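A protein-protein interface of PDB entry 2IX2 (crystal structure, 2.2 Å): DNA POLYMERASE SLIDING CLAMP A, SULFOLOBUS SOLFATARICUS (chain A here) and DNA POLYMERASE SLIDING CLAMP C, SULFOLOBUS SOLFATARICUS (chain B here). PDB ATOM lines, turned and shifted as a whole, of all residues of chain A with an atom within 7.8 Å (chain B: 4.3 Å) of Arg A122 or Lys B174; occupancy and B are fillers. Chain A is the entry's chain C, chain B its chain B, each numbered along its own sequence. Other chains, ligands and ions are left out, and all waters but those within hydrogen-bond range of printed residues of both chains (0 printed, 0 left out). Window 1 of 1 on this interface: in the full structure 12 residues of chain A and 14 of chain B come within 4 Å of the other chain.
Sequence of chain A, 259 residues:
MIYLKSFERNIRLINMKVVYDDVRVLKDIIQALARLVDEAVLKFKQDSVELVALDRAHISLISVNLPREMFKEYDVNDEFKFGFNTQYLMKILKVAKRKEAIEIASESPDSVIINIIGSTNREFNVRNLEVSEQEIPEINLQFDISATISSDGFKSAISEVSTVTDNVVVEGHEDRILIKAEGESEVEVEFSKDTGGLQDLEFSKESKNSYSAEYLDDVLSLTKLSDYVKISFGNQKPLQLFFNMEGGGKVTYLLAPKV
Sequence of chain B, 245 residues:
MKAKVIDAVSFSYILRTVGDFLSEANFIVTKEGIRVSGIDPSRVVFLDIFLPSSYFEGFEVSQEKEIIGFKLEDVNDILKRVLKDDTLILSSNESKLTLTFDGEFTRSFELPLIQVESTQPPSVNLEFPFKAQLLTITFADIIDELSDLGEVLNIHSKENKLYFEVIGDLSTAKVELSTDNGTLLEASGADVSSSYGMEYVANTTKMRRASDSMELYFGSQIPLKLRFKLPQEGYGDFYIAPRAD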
ATOM      1  N   ILE A  92      17.312 -35.703  -6.486  1.00  0.00           N
ATOM      2  CA  ILE A  92      16.778 -34.415  -6.048  1.00  0.00           C
ATOM      3  C   ILE A  92      17.014 -33.349  -7.133  1.00  0.00           C
ATOM      4  O   ILE A  92      16.073 -32.670  -7.555  1.00  0.00           O
ATOM      5  CB  ILE A  92      17.369 -33.968  -4.680  1.00  0.00           C
ATOM      6  CG1 ILE A  92      16.795 -34.838  -3.564  1.00  0.00           C
ATOM      7  CG2 ILE A  92      17.062 -32.485  -4.406  1.00  0.00           C
ATOM      8  CD1 ILE A  92      17.513 -34.659  -2.269  1.00  0.00           C
ATOM      9  N   VAL A  95      14.591 -33.266 -10.085  1.00  0.00           N
ATOM     10  CA  VAL A  95      13.302 -32.616  -9.890  1.00  0.00           C
ATOM     11  C   VAL A  95      13.191 -31.236 -10.565  1.00  0.00           C
ATOM     12  O   VAL A  95      12.113 -30.866 -11.048  1.00  0.00           O
ATOM     13  CB  VAL A  95      12.940 -32.536  -8.375  1.00  0.00           C
ATOM     14  CG1 VAL A  95      11.683 -31.700  -8.134  1.00  0.00           C
ATOM     15  CG2 VAL A  95      12.750 -33.966  -7.802  1.00  0.00           C
ATOM     16  N   ALA A  96      14.294 -30.487 -10.614  1.00  0.00           N
ATOM     17  CA  ALA A  96      14.270 -29.115 -11.138  1.00  0.00           C
ATOM     18  C   ALA A  96      13.967 -29.018 -12.638  1.00  0.00           C
ATOM     19  O   ALA A  96      14.486 -29.788 -13.448  1.00  0.00           O
ATOM     20  CB  ALA A  96      15.606 -28.387 -10.807  1.00  0.00           C
ATOM     21  N   LYS A  97      13.121 -28.057 -12.987  1.00  0.00           N
ATOM     22  CA  LYS A  97      12.855 -27.722 -14.391  1.00  0.00           C
ATOM     23  C   LYS A  97      13.761 -26.574 -14.861  1.00  0.00           C
ATOM     24  O   LYS A  97      14.427 -25.931 -14.057  1.00  0.00           O
ATOM     25  CB  LYS A  97      11.372 -27.394 -14.616  1.00  0.00           C
ATOM     26  CG  LYS A  97      10.447 -28.587 -14.384  1.00  0.00           C
ATOM     27  CD  LYS A  97       9.049 -28.359 -14.981  1.00  0.00           C
ATOM     28  CE  LYS A  97       8.078 -29.517 -14.680  1.00  0.00           C
ATOM     29  NZ  LYS A  97       8.709 -30.882 -14.855  1.00  0.00           N
ATOM     30  N   GLU A 100      15.047 -23.259 -12.923  1.00  0.00           N
ATOM     31  CA  GLU A 100      14.625 -23.149 -11.542  1.00  0.00           C
ATOM     32  C   GLU A 100      15.860 -23.195 -10.667  1.00  0.00           C
ATOM     33  O   GLU A 100      16.788 -23.956 -10.929  1.00  0.00           O
ATOM     34  CB  GLU A 100      13.693 -24.297 -11.160  1.00  0.00           C
ATOM     35  CG  GLU A 100      12.250 -24.108 -11.637  1.00  0.00           C
ATOM     36  CD  GLU A 100      11.407 -25.353 -11.403  1.00  0.00           C
ATOM     37  OE1 GLU A 100      10.170 -25.231 -11.296  1.00  0.00           O
ATOM     38  OE2 GLU A 100      11.990 -26.450 -11.325  1.00  0.00           O
ATOM     39  N   ALA A 101      15.851 -22.388  -9.617  1.00  0.00           N
ATOM     40  CA  ALA A 101      16.911 -22.374  -8.619  1.00  0.00           C
ATOM     41  C   ALA A 101      16.786 -23.500  -7.585  1.00  0.00           C
ATOM     42  O   ALA A 101      15.738 -24.131  -7.434  1.00  0.00           O
ATOM     43  CB  ALA A 101      16.950 -21.009  -7.921  1.00  0.00           C
ATOM     44  N   ILE A 102      17.885 -23.733  -6.880  1.00  0.00           N
ATOM     45  CA  ILE A 102      17.931 -24.619  -5.753  1.00  0.00           C
ATOM     46  C   ILE A 102      18.474 -23.863  -4.532  1.00  0.00           C
ATOM     47  O   ILE A 102      19.421 -23.040  -4.634  1.00  0.00           O
ATOM     48  CB  ILE A 102      18.768 -25.913  -6.036  1.00  0.00           C
ATOM     49  CG1 ILE A 102      18.761 -26.830  -4.810  1.00  0.00           C
ATOM     50  CG2 ILE A 102      20.213 -25.567  -6.462  1.00  0.00           C
ATOM     51  CD1 ILE A 102      19.443 -28.227  -5.007  1.00  0.00           C
ATOM     52  N   GLU A 103      17.846 -24.146  -3.389  1.00  0.00           N
ATOM     53  CA  GLU A 103      18.242 -23.603  -2.120  1.00  0.00           C
ATOM     54  C   GLU A 103      18.705 -24.755  -1.272  1.00  0.00           C
ATOM     55  O   GLU A 103      18.031 -25.784  -1.209  1.00  0.00           O
ATOM     56  CB  GLU A 103      17.060 -22.876  -1.454  1.00  0.00           C
ATOM     57  CG  GLU A 103      17.363 -22.398  -0.039  1.00  0.00           C
ATOM     58  CD  GLU A 103      16.137 -21.900   0.730  1.00  0.00           C
ATOM     59  OE1 GLU A 103      16.365 -21.329   1.825  1.00  0.00           O
ATOM     60  OE2 GLU A 103      14.966 -22.078   0.271  1.00  0.00           O
ATOM     61  N   ILE A 113      17.922 -28.766   4.539  1.00  0.00           N
ATOM     62  CA  ILE A 113      16.745 -28.555   3.725  1.00  0.00           C
ATOM     63  C   ILE A 113      17.132 -28.188   2.297  1.00  0.00           C
ATOM     64  O   ILE A 113      17.917 -27.246   2.084  1.00  0.00           O
ATOM     65  CB  ILE A 113      15.771 -27.560   4.376  1.00  0.00           C
ATOM     66  CG1 ILE A 113      15.330 -28.139   5.746  1.00  0.00           C
ATOM     67  CG2 ILE A 113      14.564 -27.312   3.435  1.00  0.00           C
ATOM     68  CD1 ILE A 113      13.994 -27.643   6.283  1.00  0.00           C
ATOM     69  N   ILE A 114      16.660 -28.982   1.332  1.00  0.00           N
ATOM     70  CA  ILE A 114      16.807 -28.615  -0.081  1.00  0.00           C
ATOM     71  C   ILE A 114      15.464 -28.249  -0.733  1.00  0.00           C
ATOM     72  O   ILE A 114      14.534 -29.063  -0.769  1.00  0.00           O
ATOM     73  CB  ILE A 114      17.543 -29.714  -0.895  1.00  0.00           C
ATOM     74  CG1 ILE A 114      18.856 -30.062  -0.228  1.00  0.00           C
ATOM     75  CG2 ILE A 114      17.801 -29.255  -2.317  1.00  0.00           C
ATOM     76  CD1 ILE A 114      19.620 -31.121  -0.904  1.00  0.00           C
ATOM     77  N   ASN A 115      15.357 -27.001  -1.200  1.00  0.00           N
ATOM     78  CA  ASN A 115      14.168 -26.547  -1.918  1.00  0.00           C
ATOM     79  C   ASN A 115      14.454 -26.379  -3.403  1.00  0.00           C
ATOM     80  O   ASN A 115      15.408 -25.689  -3.791  1.00  0.00           O
ATOM     81  CB  ASN A 115      13.626 -25.213  -1.352  1.00  0.00           C
ATOM     82  CG  ASN A 115      13.052 -25.353   0.054  1.00  0.00           C
ATOM     83  OD1 ASN A 115      12.351 -26.308   0.348  1.00  0.00           O
ATOM     84  ND2 ASN A 115      13.333 -24.382   0.917  1.00  0.00           N
ATOM     85  N   ILE A 116      13.640 -27.022  -4.232  1.00  0.00           N
ATOM     86  CA  ILE A 116      13.655 -26.764  -5.646  1.00  0.00           C
ATOM     87  C   ILE A 116      12.617 -25.666  -5.855  1.00  0.00           C
ATOM     88  O   ILE A 116      11.408 -25.875  -5.612  1.00  0.00           O
ATOM     89  CB  ILE A 116      13.342 -28.022  -6.482  1.00  0.00           C
ATOM     90  CG1 ILE A 116      14.346 -29.162  -6.195  1.00  0.00           C
ATOM     91  CG2 ILE A 116      13.297 -27.688  -7.970  1.00  0.00           C
ATOM     92  CD1 ILE A 116      15.835 -28.793  -6.291  1.00  0.00           C
ATOM     93  N   ILE A 117      13.097 -24.490  -6.269  1.00  0.00           N
ATOM     94  CA  ILE A 117      12.261 -23.289  -6.250  1.00  0.00           C
ATOM     95  C   ILE A 117      11.441 -23.121  -7.528  1.00  0.00           C
ATOM     96  O   ILE A 117      11.976 -22.900  -8.610  1.00  0.00           O
ATOM     97  CB  ILE A 117      13.078 -21.994  -5.929  1.00  0.00           C
ATOM     98  CG1 ILE A 117      13.726 -22.083  -4.548  1.00  0.00           C
ATOM     99  CG2 ILE A 117      12.184 -20.756  -5.947  1.00  0.00           C
ATOM    100  CD1 ILE A 117      15.023 -21.220  -4.423  1.00  0.00           C
ATOM    101  N   GLY A 118      10.131 -23.222  -7.382  1.00  0.00           N
ATOM    102  CA  GLY A 118       9.205 -22.964  -8.476  1.00  0.00           C
ATOM    103  C   GLY A 118       7.962 -22.329  -7.927  1.00  0.00           C
ATOM    104  O   GLY A 118       7.972 -21.836  -6.803  1.00  0.00           O
ATOM    105  N   SER A 119       6.891 -22.342  -8.717  1.00  0.00           N
ATOM    106  CA  SER A 119       5.590 -21.800  -8.295  1.00  0.00           C
ATOM    107  C   SER A 119       5.161 -22.399  -6.954  1.00  0.00           C
ATOM    108  O   SER A 119       4.583 -21.714  -6.105  1.00  0.00           O
ATOM    109  CB  SER A 119       4.530 -22.046  -9.364  1.00  0.00           C
ATOM    110  OG  SER A 119       4.480 -23.421  -9.715  1.00  0.00           O
ATOM    111  N   THR A 120       5.443 -23.685  -6.769  1.00  0.00           N
ATOM    112  CA  THR A 120       5.439 -24.270  -5.442  1.00  0.00           C
ATOM    113  C   THR A 120       6.777 -24.908  -5.358  1.00  0.00           C
ATOM    114  O   THR A 120       7.277 -25.438  -6.345  1.00  0.00           O
ATOM    115  CB  THR A 120       4.343 -25.347  -5.208  1.00  0.00           C
ATOM    116  OG1 THR A 120       4.563 -26.472  -6.064  1.00  0.00           O
ATOM    117  CG2 THR A 120       2.929 -24.782  -5.445  1.00  0.00           C
ATOM    118  N   ASN A 121       7.362 -24.826  -4.177  1.00  0.00           N
ATOM    119  CA  ASN A 121       8.613 -25.449  -3.937  1.00  0.00           C
ATOM    120  C   ASN A 121       8.445 -26.955  -3.770  1.00  0.00           C
ATOM    121  O   ASN A 121       7.402 -27.441  -3.334  1.00  0.00           O
ATOM    122  CB  ASN A 121       9.292 -24.843  -2.702  1.00  0.00           C
ATOM    123  CG  ASN A 121       9.630 -23.333  -2.866  1.00  0.00           C
ATOM    124  OD1 ASN A 121      10.328 -22.784  -2.026  1.00  0.00           O
ATOM    125  ND2 ASN A 121       9.116 -22.676  -3.921  1.00  0.00           N
ATOM    126  N   ARG A 122       9.483 -27.673  -4.165  1.00  0.00           N
ATOM    127  CA  ARG A 122       9.592 -29.079  -3.846  1.00  0.00           C
ATOM    128  C   ARG A 122      10.650 -29.096  -2.754  1.00  0.00           C
ATOM    129  O   ARG A 122      11.812 -28.718  -2.981  1.00  0.00           O
ATOM    130  CB  ARG A 122       9.955 -29.919  -5.074  1.00  0.00           C
ATOM    131  CG  ARG A 122       8.854 -29.967  -6.166  1.00  0.00           C
ATOM    132  CD  ARG A 122       8.887 -28.704  -7.061  1.00  0.00           C
ATOM    133  NE  ARG A 122       8.263 -28.885  -8.369  1.00  0.00           N
ATOM    134  CZ  ARG A 122       7.032 -28.477  -8.693  1.00  0.00           C
ATOM    135  NH1 ARG A 122       6.268 -27.842  -7.805  1.00  0.00           N
ATOM    136  NH2 ARG A 122       6.560 -28.700  -9.914  1.00  0.00           N
ATOM    137  N   GLU A 123      10.201 -29.473  -1.560  1.00  0.00           N
ATOM    138  CA  GLU A 123      11.002 -29.398  -0.359  1.00  0.00           C
ATOM    139  C   GLU A 123      11.502 -30.773   0.066  1.00  0.00           C
ATOM    140  O   GLU A 123      10.706 -31.711   0.218  1.00  0.00           O
ATOM    141  CB  GLU A 123      10.153 -28.778   0.746  1.00  0.00           C
ATOM    142  CG  GLU A 123      10.871 -28.670   2.082  1.00  0.00           C
ATOM    143  CD  GLU A 123       9.878 -28.458   3.212  1.00  0.00           C
ATOM    144  OE1 GLU A 123       9.928 -29.236   4.191  1.00  0.00           O
ATOM    145  OE2 GLU A 123       9.019 -27.542   3.105  1.00  0.00           O
ATOM    146  N   PHE A 124      12.818 -30.890   0.224  1.00  0.00           N
ATOM    147  CA  PHE A 124      13.444 -32.112   0.695  1.00  0.00           C
ATOM    148  C   PHE A 124      14.058 -31.869   2.060  1.00  0.00           C
ATOM    149  O   PHE A 124      14.988 -31.060   2.198  1.00  0.00           O
ATOM    150  CB  PHE A 124      14.504 -32.645  -0.287  1.00  0.00           C
ATOM    151  CG  PHE A 124      13.941 -33.030  -1.611  1.00  0.00           C
ATOM    152  CD1 PHE A 124      13.688 -32.064  -2.569  1.00  0.00           C
ATOM    153  CD2 PHE A 124      13.612 -34.361  -1.888  1.00  0.00           C
ATOM    154  CE1 PHE A 124      13.126 -32.402  -3.795  1.00  0.00           C
ATOM    155  CE2 PHE A 124      13.076 -34.702  -3.103  1.00  0.00           C
ATOM    156  CZ  PHE A 124      12.824 -33.718  -4.064  1.00  0.00           C
ATOM    157  N   ASN A 125      13.549 -32.573   3.068  1.00  0.00           N
ATOM    158  CA  ASN A 125      14.207 -32.564   4.365  1.00  0.00           C
ATOM    159  C   ASN A 125      15.100 -33.795   4.472  1.00  0.00           C
ATOM    160  O   ASN A 125      14.606 -34.920   4.473  1.00  0.00           O
ATOM    161  CB  ASN A 125      13.159 -32.508   5.496  1.00  0.00           C
ATOM    162  CG  ASN A 125      13.772 -32.123   6.850  1.00  0.00           C
ATOM    163  OD1 ASN A 125      14.976 -31.892   6.962  1.00  0.00           O
ATOM    164  ND2 ASN A 125      12.928 -32.037   7.880  1.00  0.00           N
ATOM    165  N   ILE B 142       4.155 -32.493 -10.821  1.00  0.00           N
ATOM    166  CA  ILE B 142       4.466 -32.875  -9.440  1.00  0.00           C
ATOM    167  C   ILE B 142       4.556 -34.381  -9.259  1.00  0.00           C
ATOM    168  O   ILE B 142       5.483 -34.887  -8.617  1.00  0.00           O
ATOM    169  CB  ILE B 142       3.451 -32.264  -8.416  1.00  0.00           C
ATOM    170  CG1 ILE B 142       3.708 -30.751  -8.288  1.00  0.00           C
ATOM    171  CG2 ILE B 142       3.551 -32.990  -7.073  1.00  0.00           C
ATOM    172  CD1 ILE B 142       2.493 -29.905  -7.845  1.00  0.00           C
ATOM    173  N   GLU B 145       7.681 -35.796 -10.984  1.00  0.00           N
ATOM    174  CA  GLU B 145       8.849 -35.459 -10.151  1.00  0.00           C
ATOM    175  C   GLU B 145       8.987 -36.315  -8.883  1.00  0.00           C
ATOM    176  O   GLU B 145      10.098 -36.561  -8.425  1.00  0.00           O
ATOM    177  CB  GLU B 145       8.785 -33.991  -9.759  1.00  0.00           C
ATOM    178  CG  GLU B 145       9.030 -33.072 -10.953  1.00  0.00           C
ATOM    179  CD  GLU B 145       8.584 -31.629 -10.730  1.00  0.00           C
ATOM    180  OE1 GLU B 145       8.313 -31.241  -9.582  1.00  0.00           O
ATOM    181  OE2 GLU B 145       8.522 -30.868 -11.723  1.00  0.00           O
ATOM    182  N   HIS B 156      -1.966 -35.459   2.396  1.00  0.00           N
ATOM    183  CA  HIS B 156      -2.733 -34.953   3.527  1.00  0.00           C
ATOM    184  C   HIS B 156      -3.176 -33.514   3.316  1.00  0.00           C
ATOM    185  O   HIS B 156      -2.561 -32.784   2.537  1.00  0.00           O
ATOM    186  CB  HIS B 156      -1.999 -35.191   4.870  1.00  0.00           C
ATOM    187  CG  HIS B 156      -0.881 -34.238   5.147  1.00  0.00           C
ATOM    188  ND1 HIS B 156       0.397 -34.418   4.660  1.00  0.00           N
ATOM    189  CD2 HIS B 156      -0.846 -33.108   5.893  1.00  0.00           C
ATOM    190  CE1 HIS B 156       1.168 -33.425   5.082  1.00  0.00           C
ATOM    191  NE2 HIS B 156       0.437 -32.621   5.837  1.00  0.00           N
ATOM    192  N   TYR B 163      -1.124 -31.520   0.624  1.00  0.00           N
ATOM    193  CA  TYR B 163       0.276 -31.937   0.660  1.00  0.00           C
ATOM    194  C   TYR B 163       0.458 -33.286   0.006  1.00  0.00           C
ATOM    195  O   TYR B 163      -0.315 -34.225   0.274  1.00  0.00           O
ATOM    196  CB  TYR B 163       0.769 -32.010   2.101  1.00  0.00           C
ATOM    197  CG  TYR B 163       0.732 -30.682   2.790  1.00  0.00           C
ATOM    198  CD1 TYR B 163      -0.418 -30.253   3.446  1.00  0.00           C
ATOM    199  CD2 TYR B 163       1.834 -29.839   2.759  1.00  0.00           C
ATOM    200  CE1 TYR B 163      -0.460 -29.048   4.072  1.00  0.00           C
ATOM    201  CE2 TYR B 163       1.812 -28.631   3.385  1.00  0.00           C
ATOM    202  CZ  TYR B 163       0.652 -28.237   4.036  1.00  0.00           C
ATOM    203  OH  TYR B 163       0.615 -27.027   4.652  1.00  0.00           O
ATOM    204  N   PHE B 164       1.439 -33.356  -0.883  1.00  0.00           N
ATOM    205  CA  PHE B 164       1.936 -34.622  -1.436  1.00  0.00           C
ATOM    206  C   PHE B 164       3.325 -34.836  -0.845  1.00  0.00           C
ATOM    207  O   PHE B 164       4.193 -33.960  -0.964  1.00  0.00           O
ATOM    208  CB  PHE B 164       2.116 -34.536  -2.961  1.00  0.00           C
ATOM    209  CG  PHE B 164       0.840 -34.379  -3.742  1.00  0.00           C
ATOM    210  CD1 PHE B 164       0.881 -33.937  -5.056  1.00  0.00           C
ATOM    211  CD2 PHE B 164      -0.398 -34.626  -3.175  1.00  0.00           C
ATOM    212  CE1 PHE B 164      -0.297 -33.759  -5.794  1.00  0.00           C
ATOM    213  CE2 PHE B 164      -1.588 -34.456  -3.917  1.00  0.00           C
ATOM    214  CZ  PHE B 164      -1.526 -34.019  -5.216  1.00  0.00           C
ATOM    215  N   GLU B 165       3.534 -36.000  -0.237  1.00  0.00           N
ATOM    216  CA  GLU B 165       4.776 -36.317   0.432  1.00  0.00           C
ATOM    217  C   GLU B 165       5.262 -37.713   0.082  1.00  0.00           C
ATOM    218  O   GLU B 165       4.459 -38.647  -0.098  1.00  0.00           O
ATOM    219  CB  GLU B 165       4.597 -36.283   1.952  1.00  0.00           C
ATOM    220  CG  GLU B 165       4.575 -34.922   2.557  1.00  0.00           C
ATOM    221  CD  GLU B 165       4.727 -34.962   4.061  1.00  0.00           C
ATOM    222  OE1 GLU B 165       5.520 -35.791   4.580  1.00  0.00           O
ATOM    223  OE2 GLU B 165       4.082 -34.133   4.723  1.00  0.00           O
ATOM    224  N   THR B 172      12.551 -36.798   3.530  1.00  0.00           N
ATOM    225  CA  THR B 172      11.141 -36.604   3.159  1.00  0.00           C
ATOM    226  C   THR B 172      11.061 -35.565   2.051  1.00  0.00           C
ATOM    227  O   THR B 172      11.771 -34.559   2.092  1.00  0.00           O
ATOM    228  CB  THR B 172      10.266 -36.165   4.358  1.00  0.00           C
ATOM    229  OG1 THR B 172      10.199 -37.235   5.301  1.00  0.00           O
ATOM    230  CG2 THR B 172       8.836 -35.835   3.919  1.00  0.00           C
ATOM    231  N   ALA B 173      10.242 -35.841   1.046  1.00  0.00           N
ATOM    232  CA  ALA B 173       9.942 -34.874   0.001  1.00  0.00           C
ATOM    233  C   ALA B 173       8.528 -34.384   0.270  1.00  0.00           C
ATOM    234  O   ALA B 173       7.642 -35.175   0.617  1.00  0.00           O
ATOM    235  CB  ALA B 173      10.033 -35.495  -1.373  1.00  0.00           C
ATOM    236  N   LYS B 174       8.340 -33.078   0.144  1.00  0.00           N
ATOM    237  CA  LYS B 174       7.061 -32.469   0.446  1.00  0.00           C
ATOM    238  C   LYS B 174       6.737 -31.403  -0.601  1.00  0.00           C
ATOM    239  O   LYS B 174       7.609 -30.624  -1.014  1.00  0.00           O
ATOM    240  CB  LYS B 174       7.095 -31.893   1.863  1.00  0.00           C
ATOM    241  CG  LYS B 174       5.737 -31.417   2.399  1.00  0.00           C
ATOM    242  CD  LYS B 174       5.804 -31.099   3.908  1.00  0.00           C
ATOM    243  CE  LYS B 174       4.392 -31.096   4.493  1.00  0.00           C
ATOM    244  NZ  LYS B 174       4.212 -31.960   5.725  1.00  0.00           N
ATOM    245  N   VAL B 175       5.499 -31.416  -1.078  1.00  0.00           N
ATOM    246  CA  VAL B 175       4.999 -30.341  -1.942  1.00  0.00           C
ATOM    247  C   VAL B 175       3.680 -29.815  -1.335  1.00  0.00           C
ATOM    248  O   VAL B 175       2.791 -30.595  -1.008  1.00  0.00           O
ATOM    249  CB  VAL B 175       4.853 -30.773  -3.446  1.00  0.00           C
ATOM    250  CG1 VAL B 175       4.622 -29.549  -4.345  1.00  0.00           C
ATOM    251  CG2 VAL B 175       6.139 -31.563  -3.988  1.00  0.00           C
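Of the 10 printed residues of chain B, 6 touch a printed residue of chain A.
Hydrophobic or aromatic side chains of chain B that line the printed part of chain A: Ile B142, Ala B173 and Val B175.
Printed residues of chain A that touch a printed residue of chain B: Val A95, Lys A97, Thr A120, Asn A121, Arg A122, Glu A123, Phe A124 and Asn A125.
Along chain A the printed residues that touch a printed residue of chain B span positions 95 to 125.
Among the printed residues, Asp or Glu carboxylates within 4 Å of a Lys or Arg side-chain nitrogen of the other chain: Lys A97 with Glu B145 and Arg A122 with Glu B145.
The backbone carbonyl oxygen of Arg A122 lies within hydrogen-bond range of the backbone NH of Ile A116.
OG1 of Thr A120 is in hydrogen-bond range of NH1 of Arg A122 (2.8 Å).
N of Lys A97 sits at hydrogen-bond distance from OE2 of Glu A100 (2.6 Å).
The backbone carbonyl oxygen (O) of Gly A118 lies within hydrogen-bond range of the side-chain amide nitrogen (ND2) of Asn A121, at 3.2 Å.
The backbone carbonyl oxygen of Ile A114 is in hydrogen-bond range of the backbone NH of Phe A124 (2.7 Å).
The backbone carbonyl oxygen of Phe B164 sits at hydrogen-bond distance from the backbone NH of Val B175, at 2.9 Å.
Among the printed residues, merely in contact across the chains: Val A95 with Glu B145, Thr A120 with Val B175, Asn A121 with Lys B174, Asn A121 with Val B175, Arg A122 with Ile B142, Arg A122 with Lys B174, Arg A122 with Val B175, Glu A123 with Thr B172, Glu A123 with Ala B173, Phe A124 with Thr B172 and Phe A124 with Ala B173.
Lys B174 touches just these residues of chain A: Asn A121, Arg A122 and Glu A123.
Printed residues of chain B within 4 Å of Thr A120: Val B175 (3.5 Å).
Of the printed residues of chain A, Thr B172 touches Glu A123 (3.6 Å), Phe A124 (3.3 Å) and Asn A125 (2.8 Å).
Glu A100 touches none of the printed residues of chain B.
Ala A96 touches none of the printed residues of chain B.
The nearest printed residue of chain B that does not touch Arg A122 is Ala B173 (6.4 Å).
The nearest printed residue of chain B that does not touch Glu A123 is Val B175 (5.1 Å).
The side-chain carboxylate (OE2) of Glu B145 is in salt-bridge range of the side-chain amino group (NZ) of Lys A97 (3.1 Å).
The guanidinium group (NE) of Arg A122 lies within salt-bridge range of the side-chain carboxylate (OE1) of Glu B145.
N of Lys B174 sits at hydrogen-bond distance from O of Glu A123, 2.7 Å away.
O of Thr B172 is in hydrogen-bond range of N of Asn A125.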
